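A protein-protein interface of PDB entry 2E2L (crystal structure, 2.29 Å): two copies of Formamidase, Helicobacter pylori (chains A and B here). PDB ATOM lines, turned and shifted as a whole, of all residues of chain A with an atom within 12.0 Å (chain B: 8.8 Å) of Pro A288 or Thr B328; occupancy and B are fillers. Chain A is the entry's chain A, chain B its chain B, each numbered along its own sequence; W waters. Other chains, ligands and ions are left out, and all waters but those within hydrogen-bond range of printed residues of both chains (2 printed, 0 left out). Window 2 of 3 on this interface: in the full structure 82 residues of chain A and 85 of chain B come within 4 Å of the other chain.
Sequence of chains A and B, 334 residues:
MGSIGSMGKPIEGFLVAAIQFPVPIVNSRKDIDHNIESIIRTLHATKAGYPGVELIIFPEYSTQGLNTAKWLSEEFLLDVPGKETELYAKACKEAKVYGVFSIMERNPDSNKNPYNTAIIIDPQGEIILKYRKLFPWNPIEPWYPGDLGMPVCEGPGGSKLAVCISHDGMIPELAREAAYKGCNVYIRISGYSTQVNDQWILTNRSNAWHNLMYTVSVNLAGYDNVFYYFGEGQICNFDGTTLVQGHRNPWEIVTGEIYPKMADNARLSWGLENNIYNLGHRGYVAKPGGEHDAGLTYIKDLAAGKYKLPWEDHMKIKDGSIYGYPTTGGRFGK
A ring nitrogen (ND1) of His A281 sits at hydrogen-bond distance from the backbone carbonyl oxygen (O) of Tyr A277 (3.3 Å). O of Arg A282 is in hydrogen-bond range of N of Glu A291. N of Phe B332 lies within hydrogen-bond range of OD1 of Asn B113 (3.1 Å). OD1 of Asp B319 lies within hydrogen-bond range of OG of Ser B321, 2.8 Å away. The backbone NH (N) of Tyr B325 is in hydrogen-bond range of the backbone carbonyl oxygen (O) of Gly B320 (3.0 Å). The guanidinium group of Arg A282 lies within hydrogen-bond range of the backbone carbonyl oxygen of Asp A293 (2.9 Å).
Among the printed residues, pairs that only touch across the chains: Tyr A277 with Lys B318 (3.3 Å), Arg A282 with Pro B145 (3.3 Å), Gly A283 with Pro B145 (3.7 Å), Tyr A284 with Lys B318 (3.3 Å), Tyr A284 with Asp B319 (3.5 Å), Val A285 with Gly B320 (3.8 Å), Val A285 with Phe B332 (3.7 Å), Ala A286 with Asn B113 (3.6 Å), Ala A286 with Tyr B144 (3.7 Å), Lys A287 with Tyr B144 (3.6 Å), Pro A288 with Thr B327 (3.4 Å), Pro A288 with Thr B328 (3.8 Å) and Pro A288 with Gly B329 (3.7 Å).
Pro A288 touches three residues of chain B. Of chain A, only Pro A288 comes within 4 Å of Thr B328. No residue of chain B comes within 4 Å of Gly A289. No residue of chain A comes within 4 Å of Pro B326. Gly B329 touches just one residue of chain A: Pro A288. No residue of chain A comes within 4 Å of Gly B330. Of the printed residues of chain A, Asp B319 touches Tyr A284. Printed residues of chain B within 4 Å of Gly A283: Pro B145 (3.7 Å). The nearest residue of chain B that does not touch Pro A288 is Gly B330 (5.2 Å). The nearest residue of chain A that does not touch Thr B328 is Val A285 (6.4 Å). The nearest printed residue of chain B that does not touch Arg A282 is Tyr B144 (6.1 Å).
Of the 15 printed residues of chain B, 10 touch a printed residue of chain A. Hydrophobic or aromatic side chains of chain B that line the printed part of chain A: Tyr B144, Pro B145 and Phe B332. Of the 16 printed residues of chain A, 8 touch a printed residue of chain B. Among the printed residues, 13 pairs touch across the chains.
No position is printed for both chains. Of the 13 pairs that touch across the chains among the printed residues, none has its exchanged pair printed and touching as well.
Water W1 bridges OH of Tyr A277 (2.7 Å) and O of Lys B318 (3.3 Å). Water W2 lies within hydrogen-bond range of the backbone carbonyl oxygen (O) of Ala A286 (2.7 Å), the backbone carbonyl oxygen (O) of Gly B330 (2.7 Å) and the backbone NH (N) of Asn B113 (2.9 Å).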
ATOM      1  N   TYR A 277      22.328 -40.602   3.814  1.00  0.00           N
ATOM      2  CA  TYR A 277      22.504 -39.152   3.822  1.00  0.00           C
ATOM      3  C   TYR A 277      22.925 -38.656   5.205  1.00  0.00           C
ATOM      4  O   TYR A 277      23.794 -37.791   5.322  1.00  0.00           O
ATOM      5  CB  TYR A 277      21.225 -38.447   3.363  1.00  0.00           C
ATOM      6  CG  TYR A 277      21.319 -36.937   3.366  1.00  0.00           C
ATOM      7  CD1 TYR A 277      22.027 -36.261   2.371  1.00  0.00           C
ATOM      8  CD2 TYR A 277      20.697 -36.181   4.363  1.00  0.00           C
ATOM      9  CE1 TYR A 277      22.117 -34.873   2.368  1.00  0.00           C
ATOM     10  CE2 TYR A 277      20.780 -34.791   4.367  1.00  0.00           C
ATOM     11  CZ  TYR A 277      21.493 -34.147   3.366  1.00  0.00           C
ATOM     12  OH  TYR A 277      21.583 -32.776   3.364  1.00  0.00           O
ATOM     13  N   ASN A 278      22.304 -39.222   6.239  1.00  0.00           N
ATOM     14  CA  ASN A 278      22.571 -38.858   7.631  1.00  0.00           C
ATOM     15  C   ASN A 278      24.028 -39.059   8.058  1.00  0.00           C
ATOM     16  O   ASN A 278      24.538 -38.312   8.895  1.00  0.00           O
ATOM     17  CB  ASN A 278      21.631 -39.624   8.571  1.00  0.00           C
ATOM     18  CG  ASN A 278      20.156 -39.374   8.268  1.00  0.00           C
ATOM     19  OD1 ASN A 278      19.759 -38.269   7.896  1.00  0.00           O
ATOM     20  ND2 ASN A 278      19.339 -40.408   8.429  1.00  0.00           N
ATOM     21  N   GLY A 280      26.748 -38.352   6.522  1.00  0.00           N
ATOM     22  CA  GLY A 280      27.563 -37.180   6.215  1.00  0.00           C
ATOM     23  C   GLY A 280      27.012 -35.849   6.698  1.00  0.00           C
ATOM     24  O   GLY A 280      27.715 -34.838   6.654  1.00  0.00           O
ATOM     25  N   HIS A 281      25.760 -35.845   7.158  1.00  0.00           N
ATOM     26  CA  HIS A 281      25.086 -34.608   7.568  1.00  0.00           C
ATOM     27  C   HIS A 281      24.350 -34.751   8.904  1.00  0.00           C
ATOM     28  O   HIS A 281      23.140 -34.517   8.985  1.00  0.00           O
ATOM     29  CB  HIS A 281      24.129 -34.136   6.468  1.00  0.00           C
ATOM     30  CG  HIS A 281      24.794 -33.912   5.146  1.00  0.00           C
ATOM     31  ND1 HIS A 281      24.987 -34.924   4.231  1.00  0.00           N
ATOM     32  CD2 HIS A 281      25.319 -32.796   4.587  1.00  0.00           C
ATOM     33  CE1 HIS A 281      25.601 -34.441   3.166  1.00  0.00           C
ATOM     34  NE2 HIS A 281      25.810 -33.151   3.355  1.00  0.00           N
ATOM     35  N   ARG A 282      25.102 -35.117   9.943  1.00  0.00           N
ATOM     36  CA  ARG A 282      24.584 -35.353  11.297  1.00  0.00           C
ATOM     37  C   ARG A 282      23.736 -34.207  11.833  1.00  0.00           C
ATOM     38  O   ARG A 282      24.158 -33.050  11.798  1.00  0.00           O
ATOM     39  CB  ARG A 282      25.738 -35.555  12.278  1.00  0.00           C
ATOM     40  CG  ARG A 282      26.670 -36.711  11.988  1.00  0.00           C
ATOM     41  CD  ARG A 282      27.917 -36.588  12.846  1.00  0.00           C
ATOM     42  NE  ARG A 282      27.561 -36.293  14.230  1.00  0.00           N
ATOM     43  CZ  ARG A 282      28.339 -35.673  15.110  1.00  0.00           C
ATOM     44  NH1 ARG A 282      29.557 -35.260  14.780  1.00  0.00           N
ATOM     45  NH2 ARG A 282      27.883 -35.464  16.334  1.00  0.00           N
ATOM     46  N   GLY A 283      22.556 -34.540  12.349  1.00  0.00           N
ATOM     47  CA  GLY A 283      21.674 -33.567  12.997  1.00  0.00           C
ATOM     48  C   GLY A 283      21.494 -32.283  12.215  1.00  0.00           C
ATOM     49  O   GLY A 283      21.838 -31.204  12.703  1.00  0.00           O
ATOM     50  N   TYR A 284      20.952 -32.396  11.003  1.00  0.00           N
ATOM     51  CA  TYR A 284      20.786 -31.240  10.121  1.00  0.00           C
ATOM     52  C   TYR A 284      19.663 -30.272  10.528  1.00  0.00           C
ATOM     53  O   TYR A 284      19.572 -29.165   9.989  1.00  0.00           O
ATOM     54  CB  TYR A 284      20.672 -31.658   8.643  1.00  0.00           C
ATOM     55  CG  TYR A 284      19.516 -32.577   8.283  1.00  0.00           C
ATOM     56  CD1 TYR A 284      18.191 -32.143   8.373  1.00  0.00           C
ATOM     57  CD2 TYR A 284      19.753 -33.867   7.804  1.00  0.00           C
ATOM     58  CE1 TYR A 284      17.132 -32.979   8.029  1.00  0.00           C
ATOM     59  CE2 TYR A 284      18.699 -34.712   7.453  1.00  0.00           C
ATOM     60  CZ  TYR A 284      17.392 -34.260   7.567  1.00  0.00           C
ATOM     61  OH  TYR A 284      16.346 -35.087   7.226  1.00  0.00           O
ATOM     62  N   VAL A 285      18.829 -30.684  11.481  1.00  0.00           N
ATOM     63  CA  VAL A 285      17.749 -29.832  11.992  1.00  0.00           C
ATOM     64  C   VAL A 285      18.293 -28.746  12.932  1.00  0.00           C
ATOM     65  O   VAL A 285      18.021 -27.559  12.739  1.00  0.00           O
ATOM     66  CB  VAL A 285      16.638 -30.659  12.697  1.00  0.00           C
ATOM     67  CG1 VAL A 285      15.571 -29.743  13.292  1.00  0.00           C
ATOM     68  CG2 VAL A 285      16.007 -31.646  11.724  1.00  0.00           C
ATOM     69  N   ALA A 286      19.064 -29.162  13.938  1.00  0.00           N
ATOM     70  CA  ALA A 286      19.645 -28.235  14.913  1.00  0.00           C
ATOM     71  C   ALA A 286      20.816 -27.440  14.333  1.00  0.00           C
ATOM     72  O   ALA A 286      21.088 -26.316  14.759  1.00  0.00           O
ATOM     73  CB  ALA A 286      20.081 -28.985  16.157  1.00  0.00           C
ATOM     74  N   LYS A 287      21.503 -28.042  13.365  1.00  0.00           N
ATOM     75  CA  LYS A 287      22.621 -27.411  12.678  1.00  0.00           C
ATOM     76  C   LYS A 287      22.423 -27.612  11.173  1.00  0.00           C
ATOM     77  O   LYS A 287      22.680 -28.703  10.664  1.00  0.00           O
ATOM     78  CB  LYS A 287      23.944 -28.024  13.153  1.00  0.00           C
ATOM     79  CG  LYS A 287      25.203 -27.439  12.521  1.00  0.00           C
ATOM     80  CD  LYS A 287      26.444 -28.198  12.980  1.00  0.00           C
ATOM     81  CE  LYS A 287      27.671 -27.842  12.150  1.00  0.00           C
ATOM     82  NZ  LYS A 287      28.195 -26.474  12.435  1.00  0.00           N
ATOM     83  N   PRO A 288      21.953 -26.565  10.461  1.00  0.00           N
ATOM     84  CA  PRO A 288      21.624 -26.662   9.033  1.00  0.00           C
ATOM     85  C   PRO A 288      22.777 -27.214   8.198  1.00  0.00           C
ATOM     86  O   PRO A 288      23.925 -26.799   8.368  1.00  0.00           O
ATOM     87  CB  PRO A 288      21.320 -25.213   8.643  1.00  0.00           C
ATOM     88  CG  PRO A 288      20.879 -24.574   9.904  1.00  0.00           C
ATOM     89  CD  PRO A 288      21.711 -25.204  10.978  1.00  0.00           C
ATOM     90  N   GLY A 289      22.462 -28.155   7.313  1.00  0.00           N
ATOM     91  CA  GLY A 289      23.475 -28.838   6.514  1.00  0.00           C
ATOM     92  C   GLY A 289      24.135 -29.983   7.262  1.00  0.00           C
ATOM     93  O   GLY A 289      24.804 -30.817   6.656  1.00  0.00           O
ATOM     94  N   GLY A 290      23.959 -30.009   8.582  1.00  0.00           N
ATOM     95  CA  GLY A 290      24.485 -31.076   9.427  1.00  0.00           C
ATOM     96  C   GLY A 290      25.971 -30.980   9.712  1.00  0.00           C
ATOM     97  O   GLY A 290      26.695 -30.232   9.051  1.00  0.00           O
ATOM     98  N   GLU A 291      26.421 -31.738  10.710  1.00  0.00           N
ATOM     99  CA  GLU A 291      27.843 -31.858  11.010  1.00  0.00           C
ATOM    100  C   GLU A 291      28.488 -32.823  10.018  1.00  0.00           C
ATOM    101  O   GLU A 291      28.057 -33.972   9.887  1.00  0.00           O
ATOM    102  CB  GLU A 291      28.063 -32.321  12.455  1.00  0.00           C
ATOM    103  CG  GLU A 291      29.530 -32.413  12.878  1.00  0.00           C
ATOM    104  CD  GLU A 291      30.288 -31.109  12.694  1.00  0.00           C
ATOM    105  OE1 GLU A 291      29.933 -30.108  13.359  1.00  0.00           O
ATOM    106  OE2 GLU A 291      31.242 -31.088  11.884  1.00  0.00           O
ATOM    107  N   HIS A 292      29.512 -32.342   9.316  1.00  0.00           N
ATOM    108  CA  HIS A 292      30.164 -33.119   8.260  1.00  0.00           C
ATOM    109  C   HIS A 292      31.187 -34.114   8.797  1.00  0.00           C
ATOM    110  O   HIS A 292      31.420 -35.160   8.188  1.00  0.00           O
ATOM    111  CB  HIS A 292      30.803 -32.197   7.219  1.00  0.00           C
ATOM    112  CG  HIS A 292      29.834 -31.259   6.568  1.00  0.00           C
ATOM    113  ND1 HIS A 292      30.116 -29.927   6.353  1.00  0.00           N
ATOM    114  CD2 HIS A 292      28.579 -31.458   6.099  1.00  0.00           C
ATOM    115  CE1 HIS A 292      29.080 -29.348   5.771  1.00  0.00           C
ATOM    116  NE2 HIS A 292      28.134 -30.255   5.608  1.00  0.00           N
ATOM    117  N   ASP A 293      31.798 -33.779   9.929  1.00  0.00           N
ATOM    118  CA  ASP A 293      32.707 -34.694  10.605  1.00  0.00           C
ATOM    119  C   ASP A 293      31.900 -35.685  11.440  1.00  0.00           C
ATOM    120  O   ASP A 293      31.259 -35.306  12.429  1.00  0.00           O
ATOM    121  CB  ASP A 293      33.704 -33.930  11.481  1.00  0.00           C
ATOM    122  CG  ASP A 293      34.868 -34.796  11.931  1.00  0.00           C
ATOM    123  OD1 ASP A 293      34.849 -35.258  13.092  1.00  0.00           O
ATOM    124  OD2 ASP A 293      35.794 -35.024  11.119  1.00  0.00           O
ATOM    125  N   ASN B 113      21.000 -26.037  20.272  1.00  0.00           N
ATOM    126  CA  ASN B 113      19.950 -26.892  20.825  1.00  0.00           C
ATOM    127  C   ASN B 113      20.487 -27.935  21.806  1.00  0.00           C
ATOM    128  O   ASN B 113      21.676 -28.254  21.776  1.00  0.00           O
ATOM    129  CB  ASN B 113      19.166 -27.573  19.697  1.00  0.00           C
ATOM    130  CG  ASN B 113      18.098 -26.674  19.102  1.00  0.00           C
ATOM    131  OD1 ASN B 113      17.698 -25.674  19.704  1.00  0.00           O
ATOM    132  ND2 ASN B 113      17.623 -27.032  17.917  1.00  0.00           N
ATOM    133  N   TYR B 144      20.870 -31.394  18.999  1.00  0.00           N
ATOM    134  CA  TYR B 144      22.156 -31.052  18.406  1.00  0.00           C
ATOM    135  C   TYR B 144      23.020 -32.308  18.303  1.00  0.00           C
ATOM    136  O   TYR B 144      23.083 -33.089  19.255  1.00  0.00           O
ATOM    137  CB  TYR B 144      22.863 -29.979  19.242  1.00  0.00           C
ATOM    138  CG  TYR B 144      23.767 -29.071  18.437  1.00  0.00           C
ATOM    139  CD1 TYR B 144      23.259 -27.931  17.815  1.00  0.00           C
ATOM    140  CD2 TYR B 144      25.126 -29.352  18.292  1.00  0.00           C
ATOM    141  CE1 TYR B 144      24.080 -27.092  17.069  1.00  0.00           C
ATOM    142  CE2 TYR B 144      25.957 -28.518  17.548  1.00  0.00           C
ATOM    143  CZ  TYR B 144      25.424 -27.392  16.941  1.00  0.00           C
ATOM    144  OH  TYR B 144      26.230 -26.560  16.204  1.00  0.00           O
ATOM    145  N   PRO B 145      23.672 -32.518  17.142  1.00  0.00           N
ATOM    146  CA  PRO B 145      24.583 -33.655  16.973  1.00  0.00           C
ATOM    147  C   PRO B 145      25.674 -33.660  18.040  1.00  0.00           C
ATOM    148  O   PRO B 145      26.309 -32.631  18.281  1.00  0.00           O
ATOM    149  CB  PRO B 145      25.183 -33.429  15.575  1.00  0.00           C
ATOM    150  CG  PRO B 145      24.885 -32.003  15.237  1.00  0.00           C
ATOM    151  CD  PRO B 145      23.591 -31.702  15.919  1.00  0.00           C
ATOM    152  N   LYS B 318      15.808 -31.970   3.727  1.00  0.00           N
ATOM    153  CA  LYS B 318      17.130 -31.620   4.251  1.00  0.00           C
ATOM    154  C   LYS B 318      17.025 -30.647   5.433  1.00  0.00           C
ATOM    155  O   LYS B 318      18.018 -30.030   5.839  1.00  0.00           O
ATOM    156  CB  LYS B 318      18.020 -31.040   3.141  1.00  0.00           C
ATOM    157  CG  LYS B 318      18.420 -32.047   2.061  1.00  0.00           C
ATOM    158  CD  LYS B 318      19.489 -31.497   1.122  1.00  0.00           C
ATOM    159  CE  LYS B 318      18.902 -30.609   0.036  1.00  0.00           C
ATOM    160  NZ  LYS B 318      19.949 -30.100  -0.890  1.00  0.00           N
ATOM    161  N   ASP B 319      15.813 -30.524   5.976  1.00  0.00           N
ATOM    162  CA  ASP B 319      15.534 -29.714   7.165  1.00  0.00           C
ATOM    163  C   ASP B 319      14.303 -30.248   7.904  1.00  0.00           C
ATOM    164  O   ASP B 319      13.616 -31.143   7.408  1.00  0.00           O
ATOM    165  CB  ASP B 319      15.357 -28.229   6.800  1.00  0.00           C
ATOM    166  CG  ASP B 319      14.264 -27.994   5.762  1.00  0.00           C
ATOM    167  OD1 ASP B 319      13.166 -28.583   5.877  1.00  0.00           O
ATOM    168  OD2 ASP B 319      14.502 -27.195   4.829  1.00  0.00           O
ATOM    169  N   GLY B 320      14.022 -29.687   9.079  1.00  0.00           N
ATOM    170  CA  GLY B 320      12.905 -30.141   9.907  1.00  0.00           C
ATOM    171  C   GLY B 320      11.615 -29.346   9.780  1.00  0.00           C
ATOM    172  O   GLY B 320      10.775 -29.380  10.682  1.00  0.00           O
ATOM    173  N   SER B 321      11.448 -28.643   8.660  1.00  0.00           N
ATOM    174  CA  SER B 321      10.253 -27.825   8.419  1.00  0.00           C
ATOM    175  C   SER B 321       8.972 -28.655   8.332  1.00  0.00           C
ATOM    176  O   SER B 321       7.892 -28.185   8.700  1.00  0.00           O
ATOM    177  CB  SER B 321      10.420 -26.984   7.148  1.00  0.00           C
ATOM    178  OG  SER B 321      10.511 -27.806   5.996  1.00  0.00           O
ATOM    179  N   TYR B 325       9.820 -27.250  12.491  1.00  0.00           N
ATOM    180  CA  TYR B 325      11.065 -26.656  12.978  1.00  0.00           C
ATOM    181  C   TYR B 325      11.645 -25.635  11.997  1.00  0.00           C
ATOM    182  O   TYR B 325      11.578 -25.839  10.784  1.00  0.00           O
ATOM    183  CB  TYR B 325      12.099 -27.745  13.288  1.00  0.00           C
ATOM    184  CG  TYR B 325      11.705 -28.680  14.415  1.00  0.00           C
ATOM    185  CD1 TYR B 325      11.521 -28.202  15.714  1.00  0.00           C
ATOM    186  CD2 TYR B 325      11.531 -30.045  14.185  1.00  0.00           C
ATOM    187  CE1 TYR B 325      11.164 -29.057  16.752  1.00  0.00           C
ATOM    188  CE2 TYR B 325      11.174 -30.909  15.217  1.00  0.00           C
ATOM    189  CZ  TYR B 325      10.994 -30.408  16.496  1.00  0.00           C
ATOM    190  OH  TYR B 325      10.642 -31.256  17.522  1.00  0.00           O
ATOM    191  N   PRO B 326      12.207 -24.524  12.521  1.00  0.00           N
ATOM    192  CA  PRO B 326      12.853 -23.515  11.674  1.00  0.00           C
ATOM    193  C   PRO B 326      14.157 -24.010  11.042  1.00  0.00           C
ATOM    194  O   PRO B 326      14.800 -24.920  11.573  1.00  0.00           O
ATOM    195  CB  PRO B 326      13.132 -22.365  12.646  1.00  0.00           C
ATOM    196  CG  PRO B 326      13.218 -23.007  13.972  1.00  0.00           C
ATOM    197  CD  PRO B 326      12.246 -24.145  13.946  1.00  0.00           C
ATOM    198  N   THR B 327      14.530 -23.391   9.923  1.00  0.00           N
ATOM    199  CA  THR B 327      15.667 -23.824   9.109  1.00  0.00           C
ATOM    200  C   THR B 327      16.890 -22.924   9.293  1.00  0.00           C
ATOM    201  O   THR B 327      17.960 -23.193   8.740  1.00  0.00           O
ATOM    202  CB  THR B 327      15.292 -23.848   7.609  1.00  0.00           C
ATOM    203  OG1 THR B 327      14.991 -22.517   7.169  1.00  0.00           O
ATOM    204  CG2 THR B 327      14.080 -24.739   7.366  1.00  0.00           C
ATOM    205  N   THR B 328      16.716 -21.860  10.073  1.00  0.00           N
ATOM    206  CA  THR B 328      17.742 -20.832  10.268  1.00  0.00           C
ATOM    207  C   THR B 328      18.964 -21.341  11.027  1.00  0.00           C
ATOM    208  O   THR B 328      20.097 -20.958  10.720  1.00  0.00           O
ATOM    209  CB  THR B 328      17.175 -19.613  11.027  1.00  0.00           C
ATOM    210  OG1 THR B 328      16.568 -20.051  12.249  1.00  0.00           O
ATOM    211  CG2 THR B 328      16.138 -18.887  10.184  1.00  0.00           C
ATOM    212  N   GLY B 329      18.726 -22.202  12.013  1.00  0.00           N
ATOM    213  CA  GLY B 329      19.776 -22.680  12.904  1.00  0.00           C
ATOM    214  C   GLY B 329      19.693 -22.024  14.269  1.00  0.00           C
ATOM    215  O   GLY B 329      18.738 -21.300  14.564  1.00  0.00           O
ATOM    216  N   GLY B 330      20.699 -22.280  15.102  1.00  0.00           N
ATOM    217  CA  GLY B 330      20.739 -21.736  16.456  1.00  0.00           C
ATOM    218  C   GLY B 330      19.755 -22.407  17.395  1.00  0.00           C
ATOM    219  O   GLY B 330      19.242 -23.489  17.102  1.00  0.00           O
ATOM    220  N   ARG B 331      19.492 -21.753  18.524  1.00  0.00           N
ATOM    221  CA  ARG B 331      18.595 -22.279  19.549  1.00  0.00           C
ATOM    222  C   ARG B 331      17.138 -21.938  19.238  1.00  0.00           C
ATOM    223  O   ARG B 331      16.800 -20.775  19.004  1.00  0.00           O
ATOM    224  CB  ARG B 331      18.995 -21.731  20.925  1.00  0.00           C
ATOM    225  CG  ARG B 331      18.144 -22.205  22.103  1.00  0.00           C
ATOM    226  CD  ARG B 331      18.514 -23.607  22.566  1.00  0.00           C
ATOM    227  NE  ARG B 331      18.012 -23.888  23.911  1.00  0.00           N
ATOM    228  CZ  ARG B 331      16.833 -24.443  24.181  1.00  0.00           C
ATOM    229  NH1 ARG B 331      16.007 -24.790  23.201  1.00  0.00           N
ATOM    230  NH2 ARG B 331      16.477 -24.651  25.442  1.00  0.00           N
ATOM    231  N   PHE B 332      16.285 -22.961  19.234  1.00  0.00           N
ATOM    232  CA  PHE B 332      14.845 -22.778  19.044  1.00  0.00           C
ATOM    233  C   PHE B 332      14.008 -23.763  19.861  1.00  0.00           C
ATOM    234  O   PHE B 332      14.475 -24.852  20.202  1.00  0.00           O
ATOM    235  CB  PHE B 332      14.455 -22.824  17.556  1.00  0.00           C
ATOM    236  CG  PHE B 332      14.924 -24.059  16.821  1.00  0.00           C
ATOM    237  CD1 PHE B 332      14.176 -25.234  16.848  1.00  0.00           C
ATOM    238  CD2 PHE B 332      16.095 -24.031  16.066  1.00  0.00           C
ATOM    239  CE1 PHE B 332      14.599 -26.369  16.154  1.00  0.00           C
ATOM    240  CE2 PHE B 332      16.527 -25.162  15.369  1.00  0.00           C
ATOM    241  CZ  PHE B 332      15.776 -26.331  15.411  1.00  0.00           C
HETATM  242  O   HOH W   1      21.169 -31.029   5.327  1.00  0.00           O
HETATM  243  O   HOH W   2      20.662 -25.803  17.370  1.00  0.00           O
